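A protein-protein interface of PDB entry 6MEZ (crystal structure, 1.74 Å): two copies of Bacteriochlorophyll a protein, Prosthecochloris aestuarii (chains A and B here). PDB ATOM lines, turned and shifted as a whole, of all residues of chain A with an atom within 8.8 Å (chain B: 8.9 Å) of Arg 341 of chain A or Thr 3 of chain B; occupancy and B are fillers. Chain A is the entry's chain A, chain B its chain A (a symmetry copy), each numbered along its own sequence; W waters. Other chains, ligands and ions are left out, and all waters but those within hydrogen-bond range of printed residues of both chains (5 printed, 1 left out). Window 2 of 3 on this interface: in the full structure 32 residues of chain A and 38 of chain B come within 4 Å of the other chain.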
ATOM      1  N   PHE A 301     -26.731  -3.249 -20.852  1.00  0.00           N
ATOM      2  CA  PHE A 301     -27.537  -2.782 -19.731  1.00  0.00           C
ATOM      3  C   PHE A 301     -26.737  -1.868 -18.838  1.00  0.00           C
ATOM      4  O   PHE A 301     -25.502  -1.915 -18.820  1.00  0.00           O
ATOM      5  CB  PHE A 301     -28.093  -3.962 -18.898  1.00  0.00           C
ATOM      6  CG  PHE A 301     -27.031  -4.832 -18.248  1.00  0.00           C
ATOM      7  CD1 PHE A 301     -26.663  -4.642 -16.921  1.00  0.00           C
ATOM      8  CD2 PHE A 301     -26.439  -5.865 -18.955  1.00  0.00           C
ATOM      9  CE1 PHE A 301     -25.701  -5.452 -16.328  1.00  0.00           C
ATOM     10  CE2 PHE A 301     -25.484  -6.686 -18.371  1.00  0.00           C
ATOM     11  CZ  PHE A 301     -25.109  -6.478 -17.050  1.00  0.00           C
ATOM     12  N   VAL A 303     -26.505  -0.673 -14.675  1.00  0.00           N
ATOM     13  CA  VAL A 303     -26.778  -1.284 -13.384  1.00  0.00           C
ATOM     14  C   VAL A 303     -27.367  -0.291 -12.375  1.00  0.00           C
ATOM     15  O   VAL A 303     -26.844   0.809 -12.179  1.00  0.00           O
ATOM     16  CB  VAL A 303     -25.480  -1.916 -12.838  1.00  0.00           C
ATOM     17  CG1 VAL A 303     -25.615  -2.284 -11.398  1.00  0.00           C
ATOM     18  CG2 VAL A 303     -25.109  -3.155 -13.667  1.00  0.00           C
ATOM     19  N   THR A 305     -28.205  -1.033  -8.689  1.00  0.00           N
ATOM     20  CA  THR A 305     -28.083  -2.146  -7.755  1.00  0.00           C
ATOM     21  C   THR A 305     -27.558  -1.715  -6.388  1.00  0.00           C
ATOM     22  O   THR A 305     -26.607  -0.934  -6.288  1.00  0.00           O
ATOM     23  CB  THR A 305     -27.159  -3.237  -8.335  1.00  0.00           C
ATOM     24  OG1 THR A 305     -27.794  -3.855  -9.460  1.00  0.00           O
ATOM     25  CG2 THR A 305     -26.850  -4.299  -7.301  1.00  0.00           C
ATOM     26  N   PRO A 322     -14.778  -4.485  -3.522  1.00  0.00           N
ATOM     27  CA  PRO A 322     -14.999  -3.033  -3.452  1.00  0.00           C
ATOM     28  C   PRO A 322     -15.504  -2.541  -2.086  1.00  0.00           C
ATOM     29  O   PRO A 322     -16.221  -3.258  -1.374  1.00  0.00           O
ATOM     30  CB  PRO A 322     -16.063  -2.784  -4.532  1.00  0.00           C
ATOM     31  CG  PRO A 322     -15.908  -3.900  -5.484  1.00  0.00           C
ATOM     32  CD  PRO A 322     -15.489  -5.094  -4.662  1.00  0.00           C
ATOM     33  N   SER A 335     -23.370   0.549  -3.269  1.00  0.00           N
ATOM     34  CA  SER A 335     -24.059   0.922  -4.502  1.00  0.00           C
ATOM     35  C   SER A 335     -23.165   1.813  -5.362  1.00  0.00           C
ATOM     36  O   SER A 335     -22.323   2.547  -4.847  1.00  0.00           O
ATOM     37  CB  SER A 335     -25.380   1.636  -4.211  1.00  0.00           C
ATOM     38  OG  SER A 335     -25.145   2.900  -3.621  1.00  0.00           O
ATOM     39  N   GLY A 336     -23.338   1.726  -6.673  1.00  0.00           N
ATOM     40  CA  GLY A 336     -22.628   2.602  -7.585  1.00  0.00           C
ATOM     41  C   GLY A 336     -21.134   2.361  -7.610  1.00  0.00           C
ATOM     42  O   GLY A 336     -20.626   1.451  -6.957  1.00  0.00           O
ATOM     43  N   GLY A 337     -20.435   3.176  -8.391  1.00  0.00           N
ATOM     44  CA  GLY A 337     -18.985   3.138  -8.425  1.00  0.00           C
ATOM     45  C   GLY A 337     -18.401   1.770  -8.711  1.00  0.00           C
ATOM     46  O   GLY A 337     -18.852   1.058  -9.603  1.00  0.00           O
ATOM     47  N   ALA A 338     -17.395   1.394  -7.932  1.00  0.00           N
ATOM     48  CA  ALA A 338     -16.693   0.151  -8.174  1.00  0.00           C
ATOM     49  C   ALA A 338     -17.618  -1.042  -7.965  1.00  0.00           C
ATOM     50  O   ALA A 338     -17.462  -2.057  -8.636  1.00  0.00           O
ATOM     51  CB  ALA A 338     -15.471   0.047  -7.282  1.00  0.00           C
ATOM     52  N   TYR A 339     -18.591  -0.924  -7.058  1.00  0.00           N
ATOM     53  CA  TYR A 339     -19.473  -2.068  -6.804  1.00  0.00           C
ATOM     54  C   TYR A 339     -20.395  -2.331  -7.993  1.00  0.00           C
ATOM     55  O   TYR A 339     -20.596  -3.483  -8.381  1.00  0.00           O
ATOM     56  CB  TYR A 339     -20.301  -1.871  -5.537  1.00  0.00           C
ATOM     57  CG  TYR A 339     -21.299  -2.996  -5.342  1.00  0.00           C
ATOM     58  CD1 TYR A 339     -20.880  -4.280  -4.995  1.00  0.00           C
ATOM     59  CD2 TYR A 339     -22.658  -2.775  -5.532  1.00  0.00           C
ATOM     60  CE1 TYR A 339     -21.813  -5.328  -4.847  1.00  0.00           C
ATOM     61  CE2 TYR A 339     -23.577  -3.788  -5.369  1.00  0.00           C
ATOM     62  CZ  TYR A 339     -23.163  -5.053  -5.032  1.00  0.00           C
ATOM     63  OH  TYR A 339     -24.121  -6.044  -4.898  1.00  0.00           O
ATOM     64  N   ALA A 340     -20.934  -1.263  -8.577  1.00  0.00           N
ATOM     65  CA  ALA A 340     -21.752  -1.376  -9.779  1.00  0.00           C
ATOM     66  C   ALA A 340     -20.973  -2.022 -10.934  1.00  0.00           C
ATOM     67  O   ALA A 340     -21.540  -2.789 -11.717  1.00  0.00           O
ATOM     68  CB  ALA A 340     -22.291   0.004 -10.196  1.00  0.00           C
ATOM     69  N   ARG A 341     -19.681  -1.719 -11.038  1.00  0.00           N
ATOM     70  CA  ARG A 341     -18.873  -2.309 -12.102  1.00  0.00           C
ATOM     71  C   ARG A 341     -18.656  -3.790 -11.824  1.00  0.00           C
ATOM     72  O   ARG A 341     -18.631  -4.614 -12.744  1.00  0.00           O
ATOM     73  CB  ARG A 341     -17.532  -1.578 -12.253  1.00  0.00           C
ATOM     74  CG  ARG A 341     -17.676  -0.166 -12.826  1.00  0.00           C
ATOM     75  CD  ARG A 341     -16.327   0.453 -13.197  1.00  0.00           C
ATOM     76  NE  ARG A 341     -15.531   0.825 -12.026  1.00  0.00           N
ATOM     77  CZ  ARG A 341     -15.555   2.028 -11.456  1.00  0.00           C
ATOM     78  NH1 ARG A 341     -16.340   2.978 -11.941  1.00  0.00           N
ATOM     79  NH2 ARG A 341     -14.798   2.283 -10.397  1.00  0.00           N
ATOM     80  N   TRP A 342     -18.518  -4.131 -10.546  1.00  0.00           N
ATOM     81  CA  TRP A 342     -18.389  -5.529 -10.162  1.00  0.00           C
ATOM     82  C   TRP A 342     -19.697  -6.289 -10.445  1.00  0.00           C
ATOM     83  O   TRP A 342     -19.660  -7.426 -10.912  1.00  0.00           O
ATOM     84  CB  TRP A 342     -17.988  -5.669  -8.685  1.00  0.00           C
ATOM     85  CG  TRP A 342     -17.812  -7.107  -8.285  1.00  0.00           C
ATOM     86  CD1 TRP A 342     -16.710  -7.899  -8.488  1.00  0.00           C
ATOM     87  CD2 TRP A 342     -18.788  -7.929  -7.653  1.00  0.00           C
ATOM     88  NE1 TRP A 342     -16.946  -9.163  -8.005  1.00  0.00           N
ATOM     89  CE2 TRP A 342     -18.217  -9.209  -7.487  1.00  0.00           C
ATOM     90  CE3 TRP A 342     -20.093  -7.705  -7.202  1.00  0.00           C
ATOM     91  CZ2 TRP A 342     -18.902 -10.258  -6.885  1.00  0.00           C
ATOM     92  CZ3 TRP A 342     -20.778  -8.752  -6.608  1.00  0.00           C
ATOM     93  CH2 TRP A 342     -20.184 -10.012  -6.460  1.00  0.00           C
ATOM     94  N   VAL A 343     -20.848  -5.670 -10.184  1.00  0.00           N
ATOM     95  CA  VAL A 343     -22.111  -6.340 -10.461  1.00  0.00           C
ATOM     96  C   VAL A 343     -22.241  -6.625 -11.957  1.00  0.00           C
ATOM     97  O   VAL A 343     -22.619  -7.738 -12.350  1.00  0.00           O
ATOM     98  CB  VAL A 343     -23.332  -5.513  -9.977  1.00  0.00           C
ATOM     99  CG1 VAL A 343     -24.633  -6.158 -10.468  1.00  0.00           C
ATOM    100  CG2 VAL A 343     -23.326  -5.418  -8.444  1.00  0.00           C
ATOM    101  N   GLU A 344     -21.919  -5.634 -12.789  1.00  0.00           N
ATOM    102  CA  GLU A 344     -21.932  -5.831 -14.242  1.00  0.00           C
ATOM    103  C   GLU A 344     -21.039  -7.006 -14.638  1.00  0.00           C
ATOM    104  O   GLU A 344     -21.449  -7.903 -15.377  1.00  0.00           O
ATOM    105  CB  GLU A 344     -21.474  -4.562 -14.978  1.00  0.00           C
ATOM    106  CG  GLU A 344     -21.423  -4.744 -16.500  1.00  0.00           C
ATOM    107  CD  GLU A 344     -20.868  -3.525 -17.233  1.00  0.00           C
ATOM    108  OE1 GLU A 344     -20.509  -2.541 -16.570  1.00  0.00           O
ATOM    109  OE2 GLU A 344     -20.796  -3.544 -18.474  1.00  0.00           O
ATOM    110  N   HIS A 345     -19.820  -6.994 -14.107  1.00  0.00           N
ATOM    111  CA  HIS A 345     -18.811  -8.039 -14.325  1.00  0.00           C
ATOM    112  C   HIS A 345     -19.344  -9.457 -14.025  1.00  0.00           C
ATOM    113  O   HIS A 345     -19.271 -10.335 -14.879  1.00  0.00           O
ATOM    114  CB  HIS A 345     -17.598  -7.668 -13.451  1.00  0.00           C
ATOM    115  CG  HIS A 345     -16.506  -8.690 -13.381  1.00  0.00           C
ATOM    116  ND1 HIS A 345     -15.439  -8.694 -14.248  1.00  0.00           N
ATOM    117  CD2 HIS A 345     -16.251  -9.656 -12.464  1.00  0.00           C
ATOM    118  CE1 HIS A 345     -14.594  -9.656 -13.903  1.00  0.00           C
ATOM    119  NE2 HIS A 345     -15.059 -10.247 -12.818  1.00  0.00           N
ATOM    120  N   VAL A 346     -19.907  -9.690 -12.840  1.00  0.00           N
ATOM    121  CA  VAL A 346     -20.332 -11.049 -12.514  1.00  0.00           C
ATOM    122  C   VAL A 346     -21.608 -11.438 -13.273  1.00  0.00           C
ATOM    123  O   VAL A 346     -21.803 -12.612 -13.561  1.00  0.00           O
ATOM    124  CB  VAL A 346     -20.540 -11.263 -10.982  1.00  0.00           C
ATOM    125  CG1 VAL A 346     -19.214 -11.112 -10.256  1.00  0.00           C
ATOM    126  CG2 VAL A 346     -21.610 -10.319 -10.403  1.00  0.00           C
ATOM    127  N   CYS A 347     -22.447 -10.469 -13.638  1.00  0.00           N
ATOM    128  CA  CYS A 347     -23.651 -10.813 -14.401  1.00  0.00           C
ATOM    129  C   CYS A 347     -23.304 -11.299 -15.801  1.00  0.00           C
ATOM    130  O   CYS A 347     -24.095 -12.004 -16.429  1.00  0.00           O
ATOM    131  CB  CYS A 347     -24.606  -9.631 -14.507  1.00  0.00           C
ATOM    132  SG  CYS A 347     -25.496  -9.311 -12.968  1.00  0.00           S
ATOM    133  N   LYS A 348     -22.136 -10.896 -16.291  1.00  0.00           N
ATOM    134  CA  LYS A 348     -21.683 -11.277 -17.625  1.00  0.00           C
ATOM    135  C   LYS A 348     -20.750 -12.491 -17.647  1.00  0.00           C
ATOM    136  O   LYS A 348     -20.293 -12.907 -18.720  1.00  0.00           O
ATOM    137  CB  LYS A 348     -21.004 -10.078 -18.302  1.00  0.00           C
ATOM    138  CG  LYS A 348     -21.968  -8.915 -18.576  1.00  0.00           C
ATOM    139  CD  LYS A 348     -21.261  -7.758 -19.252  1.00  0.00           C
ATOM    140  CE  LYS A 348     -22.259  -6.733 -19.753  1.00  0.00           C
ATOM    141  NZ  LYS A 348     -21.574  -5.594 -20.417  1.00  0.00           N
ATOM    142  N   GLY A 350     -18.029 -12.891 -15.196  1.00  0.00           N
ATOM    143  CA  GLY A 350     -16.762 -12.642 -14.523  1.00  0.00           C
ATOM    144  C   GLY A 350     -16.675 -13.266 -13.135  1.00  0.00           C
ATOM    145  O   GLY A 350     -17.675 -13.394 -12.450  1.00  0.00           O
ATOM    146  N   THR B   3     -16.700   3.970 -18.117  1.00  0.00           N
ATOM    147  CA  THR B   3     -15.515   3.110 -18.110  1.00  0.00           C
ATOM    148  C   THR B   3     -14.669   3.295 -19.367  1.00  0.00           C
ATOM    149  O   THR B   3     -15.119   2.990 -20.470  1.00  0.00           O
ATOM    150  CB  THR B   3     -15.900   1.631 -17.999  1.00  0.00           C
ATOM    151  OG1 THR B   3     -16.690   1.422 -16.821  1.00  0.00           O
ATOM    152  CG2 THR B   3     -14.653   0.776 -17.937  1.00  0.00           C
ATOM    153  N   THR B   4     -13.449   3.801 -19.205  1.00  0.00           N
ATOM    154  CA  THR B   4     -12.588   4.085 -20.347  1.00  0.00           C
ATOM    155  C   THR B   4     -11.323   3.233 -20.270  1.00  0.00           C
ATOM    156  O   THR B   4     -10.681   3.155 -19.225  1.00  0.00           O
ATOM    157  CB  THR B   4     -12.192   5.585 -20.423  1.00  0.00           C
ATOM    158  OG1 THR B   4     -13.364   6.394 -20.580  1.00  0.00           O
ATOM    159  CG2 THR B   4     -11.271   5.837 -21.607  1.00  0.00           C
ATOM    160  N   ALA B   5     -10.985   2.571 -21.369  1.00  0.00           N
ATOM    161  CA  ALA B   5      -9.721   1.856 -21.453  1.00  0.00           C
ATOM    162  C   ALA B   5      -8.692   2.769 -22.106  1.00  0.00           C
ATOM    163  O   ALA B   5      -8.865   3.172 -23.259  1.00  0.00           O
ATOM    164  CB  ALA B   5      -9.873   0.576 -22.252  1.00  0.00           C
ATOM    165  N   HIS B   6      -7.632   3.103 -21.372  1.00  0.00           N
ATOM    166  CA  HIS B   6      -6.559   3.925 -21.925  1.00  0.00           C
ATOM    167  C   HIS B   6      -5.399   3.046 -22.326  1.00  0.00           C
ATOM    168  O   HIS B   6      -4.890   2.282 -21.503  1.00  0.00           O
ATOM    169  CB  HIS B   6      -6.078   4.969 -20.914  1.00  0.00           C
ATOM    170  CG  HIS B   6      -7.171   5.813 -20.348  1.00  0.00           C
ATOM    171  ND1 HIS B   6      -7.575   6.993 -20.932  1.00  0.00           N
ATOM    172  CD2 HIS B   6      -7.945   5.650 -19.249  1.00  0.00           C
ATOM    173  CE1 HIS B   6      -8.556   7.519 -20.219  1.00  0.00           C
ATOM    174  NE2 HIS B   6      -8.798   6.724 -19.193  1.00  0.00           N
ATOM    175  N   LYS B  28      -4.354   0.890 -19.158  1.00  0.00           N
ATOM    176  CA  LYS B  28      -4.985   1.008 -17.854  1.00  0.00           C
ATOM    177  C   LYS B  28      -6.493   1.043 -18.014  1.00  0.00           C
ATOM    178  O   LYS B  28      -7.038   1.843 -18.782  1.00  0.00           O
ATOM    179  CB  LYS B  28      -4.514   2.259 -17.115  1.00  0.00           C
ATOM    180  CG  LYS B  28      -5.141   2.399 -15.741  1.00  0.00           C
ATOM    181  N   VAL B  29      -7.177   0.160 -17.300  1.00  0.00           N
ATOM    182  CA  VAL B  29      -8.638   0.163 -17.380  1.00  0.00           C
ATOM    183  C   VAL B  29      -9.222  -0.065 -15.990  1.00  0.00           C
ATOM    184  O   VAL B  29      -8.764  -0.928 -15.244  1.00  0.00           O
ATOM    185  CB  VAL B  29      -9.148  -0.880 -18.401  1.00  0.00           C
ATOM    186  CG1 VAL B  29      -8.665  -2.279 -18.057  1.00  0.00           C
ATOM    187  CG2 VAL B  29     -10.674  -0.832 -18.532  1.00  0.00           C
ATOM    188  N   ASN B  30     -10.225   0.721 -15.621  1.00  0.00           N
ATOM    189  CA  ASN B  30     -10.761   0.636 -14.266  1.00  0.00           C
ATOM    190  C   ASN B  30     -11.936  -0.338 -14.130  1.00  0.00           C
ATOM    191  O   ASN B  30     -13.039   0.043 -13.718  1.00  0.00           O
ATOM    192  CB  ASN B  30     -11.165   2.030 -13.778  1.00  0.00           C
ATOM    193  CG  ASN B  30      -9.966   2.909 -13.479  1.00  0.00           C
ATOM    194  OD1 ASN B  30      -8.904   2.421 -13.078  1.00  0.00           O
ATOM    195  ND2 ASN B  30     -10.125   4.209 -13.668  1.00  0.00           N
ATOM    196  N   VAL B  31     -11.679  -1.599 -14.471  1.00  0.00           N
ATOM    197  CA  VAL B  31     -12.651  -2.682 -14.307  1.00  0.00           C
ATOM    198  C   VAL B  31     -12.012  -3.751 -13.444  1.00  0.00           C
ATOM    199  O   VAL B  31     -10.785  -3.845 -13.391  1.00  0.00           O
ATOM    200  CB  VAL B  31     -13.067  -3.294 -15.658  1.00  0.00           C
ATOM    201  CG1 VAL B  31     -13.756  -2.245 -16.512  1.00  0.00           C
ATOM    202  CG2 VAL B  31     -11.851  -3.869 -16.392  1.00  0.00           C
ATOM    203  N   PRO B  32     -12.823  -4.559 -12.752  1.00  0.00           N
ATOM    204  CA  PRO B  32     -12.247  -5.685 -12.007  1.00  0.00           C
ATOM    205  C   PRO B  32     -11.603  -6.731 -12.922  1.00  0.00           C
ATOM    206  O   PRO B  32     -12.125  -7.027 -14.005  1.00  0.00           O
ATOM    207  CB  PRO B  32     -13.459  -6.276 -11.274  1.00  0.00           C
ATOM    208  CG  PRO B  32     -14.649  -5.810 -12.053  1.00  0.00           C
ATOM    209  CD  PRO B  32     -14.281  -4.457 -12.572  1.00  0.00           C
ATOM    210  N   ALA B  33     -10.463  -7.264 -12.506  1.00  0.00           N
ATOM    211  CA  ALA B  33      -9.930  -8.470 -13.126  1.00  0.00           C
ATOM    212  C   ALA B  33     -10.835  -9.660 -12.771  1.00  0.00           C
ATOM    213  O   ALA B  33     -11.594  -9.602 -11.809  1.00  0.00           O
ATOM    214  CB  ALA B  33      -8.490  -8.722 -12.671  1.00  0.00           C
ATOM    215  N   SER B 256      -9.820  -5.454  -7.560  1.00  0.00           N
ATOM    216  CA  SER B 256     -11.249  -5.394  -7.868  1.00  0.00           C
ATOM    217  C   SER B 256     -11.671  -4.045  -8.474  1.00  0.00           C
ATOM    218  O   SER B 256     -12.834  -3.871  -8.842  1.00  0.00           O
ATOM    219  CB  SER B 256     -12.083  -5.687  -6.609  1.00  0.00           C
ATOM    220  OG  SER B 256     -11.801  -4.741  -5.598  1.00  0.00           O
ATOM    221  N   GLN B 257     -10.755  -3.089  -8.592  1.00  0.00           N
ATOM    222  CA  GLN B 257     -11.136  -1.813  -9.198  1.00  0.00           C
ATOM    223  C   GLN B 257     -10.233  -1.361 -10.349  1.00  0.00           C
ATOM    224  O   GLN B 257     -10.370  -0.242 -10.842  1.00  0.00           O
ATOM    225  CB  GLN B 257     -11.205  -0.715  -8.130  1.00  0.00           C
ATOM    226  CG  GLN B 257     -10.119  -0.775  -7.075  1.00  0.00           C
ATOM    227  CD  GLN B 257     -10.682  -1.035  -5.689  1.00  0.00           C
ATOM    228  OE1 GLN B 257     -11.271  -2.087  -5.430  1.00  0.00           O
ATOM    229  NE2 GLN B 257     -10.508  -0.072  -4.792  1.00  0.00           N
ATOM    230  N   GLY B 258      -9.323  -2.221 -10.794  1.00  0.00           N
ATOM    231  CA  GLY B 258      -8.592  -1.910 -12.003  1.00  0.00           C
ATOM    232  C   GLY B 258      -7.452  -2.807 -12.425  1.00  0.00           C
ATOM    233  O   GLY B 258      -6.965  -3.645 -11.673  1.00  0.00           O
ATOM    234  N   PHE B 298     -16.585  -8.634 -20.048  1.00  0.00           N
ATOM    235  CA  PHE B 298     -17.332  -8.552 -18.792  1.00  0.00           C
ATOM    236  C   PHE B 298     -17.740  -7.143 -18.376  1.00  0.00           C
ATOM    237  O   PHE B 298     -18.543  -6.996 -17.468  1.00  0.00           O
ATOM    238  CB  PHE B 298     -16.524  -9.161 -17.648  1.00  0.00           C
ATOM    239  CG  PHE B 298     -16.208 -10.627 -17.817  1.00  0.00           C
ATOM    240  CD1 PHE B 298     -14.973 -11.131 -17.420  1.00  0.00           C
ATOM    241  CD2 PHE B 298     -17.152 -11.504 -18.336  1.00  0.00           C
ATOM    242  CE1 PHE B 298     -14.681 -12.501 -17.538  1.00  0.00           C
ATOM    243  CE2 PHE B 298     -16.864 -12.865 -18.462  1.00  0.00           C
ATOM    244  CZ  PHE B 298     -15.617 -13.355 -18.063  1.00  0.00           C
ATOM    245  N   ASN B 299     -17.184  -6.113 -19.005  1.00  0.00           N
ATOM    246  CA  ASN B 299     -17.597  -4.729 -18.715  1.00  0.00           C
ATOM    247  C   ASN B 299     -17.601  -3.892 -19.980  1.00  0.00           C
ATOM    248  O   ASN B 299     -16.675  -4.007 -20.788  1.00  0.00           O
ATOM    249  CB  ASN B 299     -16.656  -4.046 -17.718  1.00  0.00           C
ATOM    250  CG  ASN B 299     -16.836  -4.524 -16.285  1.00  0.00           C
ATOM    251  OD1 ASN B 299     -16.064  -5.340 -15.803  1.00  0.00           O
ATOM    252  ND2 ASN B 299     -17.829  -3.975 -15.590  1.00  0.00           N
ATOM    253  N   ASP B 300     -18.611  -3.045 -20.142  1.00  0.00           N
ATOM    254  CA  ASP B 300     -18.615  -2.092 -21.257  1.00  0.00           C
ATOM    255  C   ASP B 300     -17.486  -1.100 -21.072  1.00  0.00           C
ATOM    256  O   ASP B 300     -17.195  -0.699 -19.943  1.00  0.00           O
ATOM    257  CB  ASP B 300     -19.938  -1.334 -21.336  1.00  0.00           C
ATOM    258  CG  ASP B 300     -21.120  -2.235 -21.569  1.00  0.00           C
ATOM    259  OD1 ASP B 300     -20.928  -3.362 -22.066  1.00  0.00           O
ATOM    260  OD2 ASP B 300     -22.249  -1.799 -21.263  1.00  0.00           O
ATOM    261  N   PHE B 301     -16.870  -0.687 -22.173  1.00  0.00           N
ATOM    262  CA  PHE B 301     -15.803   0.304 -22.109  1.00  0.00           C
ATOM    263  C   PHE B 301     -15.757   1.127 -23.373  1.00  0.00           C
ATOM    264  O   PHE B 301     -16.230   0.696 -24.431  1.00  0.00           O
ATOM    265  CB  PHE B 301     -14.424  -0.357 -21.874  1.00  0.00           C
ATOM    266  CG  PHE B 301     -13.981  -1.304 -22.977  1.00  0.00           C
ATOM    267  CD1 PHE B 301     -13.115  -0.880 -23.979  1.00  0.00           C
ATOM    268  CD2 PHE B 301     -14.395  -2.624 -22.979  1.00  0.00           C
ATOM    269  CE1 PHE B 301     -12.701  -1.756 -24.976  1.00  0.00           C
ATOM    270  CE2 PHE B 301     -13.981  -3.511 -23.963  1.00  0.00           C
ATOM    271  CZ  PHE B 301     -13.131  -3.074 -24.971  1.00  0.00           C
ATOM    272  N   THR B 302     -15.211   2.329 -23.267  1.00  0.00           N
ATOM    273  CA  THR B 302     -14.871   3.087 -24.454  1.00  0.00           C
ATOM    274  C   THR B 302     -13.362   3.098 -24.590  1.00  0.00           C
ATOM    275  O   THR B 302     -12.632   2.930 -23.609  1.00  0.00           O
ATOM    276  CB  THR B 302     -15.398   4.520 -24.412  1.00  0.00           C
ATOM    277  OG1 THR B 302     -14.839   5.207 -23.286  1.00  0.00           O
ATOM    278  CG2 THR B 302     -16.916   4.514 -24.319  1.00  0.00           C
ATOM    279  N   VAL B 303     -12.902   3.290 -25.817  1.00  0.00           N
ATOM    280  CA  VAL B 303     -11.487   3.182 -26.135  1.00  0.00           C
ATOM    281  C   VAL B 303     -10.809   4.550 -26.280  1.00  0.00           C
ATOM    282  O   VAL B 303     -11.297   5.435 -26.988  1.00  0.00           O
ATOM    283  CB  VAL B 303     -11.319   2.348 -27.423  1.00  0.00           C
ATOM    284  CG1 VAL B 303      -9.936   2.457 -27.968  1.00  0.00           C
ATOM    285  CG2 VAL B 303     -11.664   0.876 -27.145  1.00  0.00           C
ATOM    286  N   ASP B 304      -9.699   4.720 -25.561  1.00  0.00           N
ATOM    287  CA  ASP B 304      -8.824   5.883 -25.688  1.00  0.00           C
ATOM    288  C   ASP B 304      -7.432   5.350 -26.003  1.00  0.00           C
ATOM    289  O   ASP B 304      -6.640   5.094 -25.099  1.00  0.00           O
ATOM    290  CB  ASP B 304      -8.820   6.710 -24.402  1.00  0.00           C
ATOM    291  CG  ASP B 304      -7.788   7.822 -24.426  1.00  0.00           C
ATOM    292  OD1 ASP B 304      -7.185   8.100 -23.365  1.00  0.00           O
ATOM    293  OD2 ASP B 304      -7.577   8.414 -25.500  1.00  0.00           O
HETATM  294  O   HOH W   1     -23.768  -3.749 -20.582  1.00  0.00           O
HETATM  295  O   HOH W   2     -18.700  -0.738 -17.609  1.00  0.00           O
HETATM  296  O   HOH W   3     -14.927  -2.401  -9.766  1.00  0.00           O
HETATM  297  O   HOH W   4     -13.794  -0.362 -10.713  1.00  0.00           O
HETATM  298  O   HOH W   5     -14.061  -6.993 -16.243  1.00  0.00           O
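O of Arg 341 of chain A is in hydrogen-bond range of ND2 of Asn 299 of chain B (3.0 Å).
The backbone carbonyl oxygen (O) of Asn 30 of chain B lies within hydrogen-bond range of the guanidinium group (NE) of Arg 341 of chain A (3.1 Å).
N of Asp 300 of chain B sits at hydrogen-bond distance from OE2 of Glu 344 of chain A (2.8 Å).
The side-chain amino group (NZ) of Lys 348 of chain A is in salt-bridge range of the side-chain carboxylate (OD1) of Asp 300 of chain B.
OE1 of Glu 344 of chain A is in hydrogen-bond range of ND2 of Asn 299 of chain B.
Ser 256 of chain B touches Pro 322 of chain A.
Arg 341 of chain A touches Thr 3 of chain B (CD to OG1, 3.8 Å).
Glu 344 of chain A touches Phe 298 of chain B (O to O, 3.7 Å).
His 345 of chain A touches Pro 32 of chain B.
His 345 of chain A touches Ala 33 of chain B (CE1 to O, 3.7 Å).
Phe 298 of chain B touches His 345 of chain A (O to CA, 3.3 Å).
His 345 of chain A touches Asn 299 of chain B (CB to OD1, 3.6 Å).
Phe 298 of chain B touches Lys 348 of chain A.
Phe 298 of chain B touches Gly 350 of chain A.
Water W4 lies within hydrogen-bond range of the guanidinium group (NE) of Arg 341 of chain A (2.5 Å), the backbone carbonyl oxygen (O) of Asn 30 of chain B (3.1 Å) and the backbone carbonyl oxygen (O) of Gln 257 of chain B (3.4 Å).
Water W1 lies within hydrogen-bond range of OD2 of Asp 300 of chain B, NZ of Lys 348 of chain A and N of Phe 301 of chain A.
Water W5 lies within hydrogen-bond range of OD1 of Asn 299 of chain B, O of Pro 32 of chain B and ND1 of His 345 of chain A.
Water W3 bridges O of Ser 256 of chain B and O of Ala 338 of chain A.
Water W2 lies within hydrogen-bond range of OE1 of Glu 344 of chain A (2.8 Å), O of Asp 300 of chain B (2.8 Å) and OG1 of Thr 3 of chain B (3.1 Å).
Of the 19 printed residues of chain A, 6 touch a printed residue of chain B.
Printed residues of chain A that touch a printed residue of chain B: Pro 322, Arg 341, Glu 344, His 345, Lys 348 and Gly 350.
Along chain A the printed residues that touch a printed residue of chain B span positions 322 to 350.
Printed residues of chain B that touch a printed residue of chain A: Thr 3, Asn 30, Pro 32, Ala 33, Ser 256, Phe 298, Asn 299 and Asp 300.
Among the printed residues, Asp or Glu carboxylates within 4 Å of a Lys or Arg side-chain nitrogen of the other chain: Lys 348 of chain A with Asp 300 of chain B.
Of the printed residues of chain B, Arg 341 of chain A touches Thr 3 (3.8 Å), Asn 30 (3.1 Å) and Asn 299 (3.0 Å).
Of the printed residues of chain A, Thr 3 of chain B touches Arg 341 (3.8 Å).
No residue of chain B comes within 4 Å of Ala 340 of chain A.
Printed residues of chain A within 4 Å of Asn 299 of chain B: Arg 341 (3.0 Å), Glu 344 (3.2 Å) and His 345 (3.6 Å).
Of the printed residues of chain A, Ala 33 of chain B touches His 345 (3.7 Å).
Printed residues of chain B within 4 Å of His 345 of chain A: Pro 32 (3.6 Å), Ala 33 (3.7 Å), Phe 298 (3.3 Å) and Asn 299 (3.6 Å).
Printed residues of chain A within 4 Å of Phe 298 of chain B: Glu 344, His 345, Lys 348 and Gly 350.
His 6 of chain B touches none of the printed residues of chain A.
The nearest printed residue of chain A that does not touch Thr 3 of chain B is Glu 344 of chain A (5.5 Å).
2 positions are printed for both chains.
O of His 345 of chain A is in hydrogen-bond range of N of Gly 350 of chain A, 2.9 Å away.
The side-chain carboxylate (OE2) of Glu 344 of chain A is in salt-bridge range of the side-chain amino group (NZ) of Lys 348 of chain A (2.9 Å).
N of Thr 302 of chain B is in hydrogen-bond range of O of Thr 3 of chain B (2.9 Å).
The side-chain hydroxyl (OG) of Ser 256 of chain B is in hydrogen-bond range of the side-chain amide oxygen (OE1) of Gln 257 of chain B (2.7 Å).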
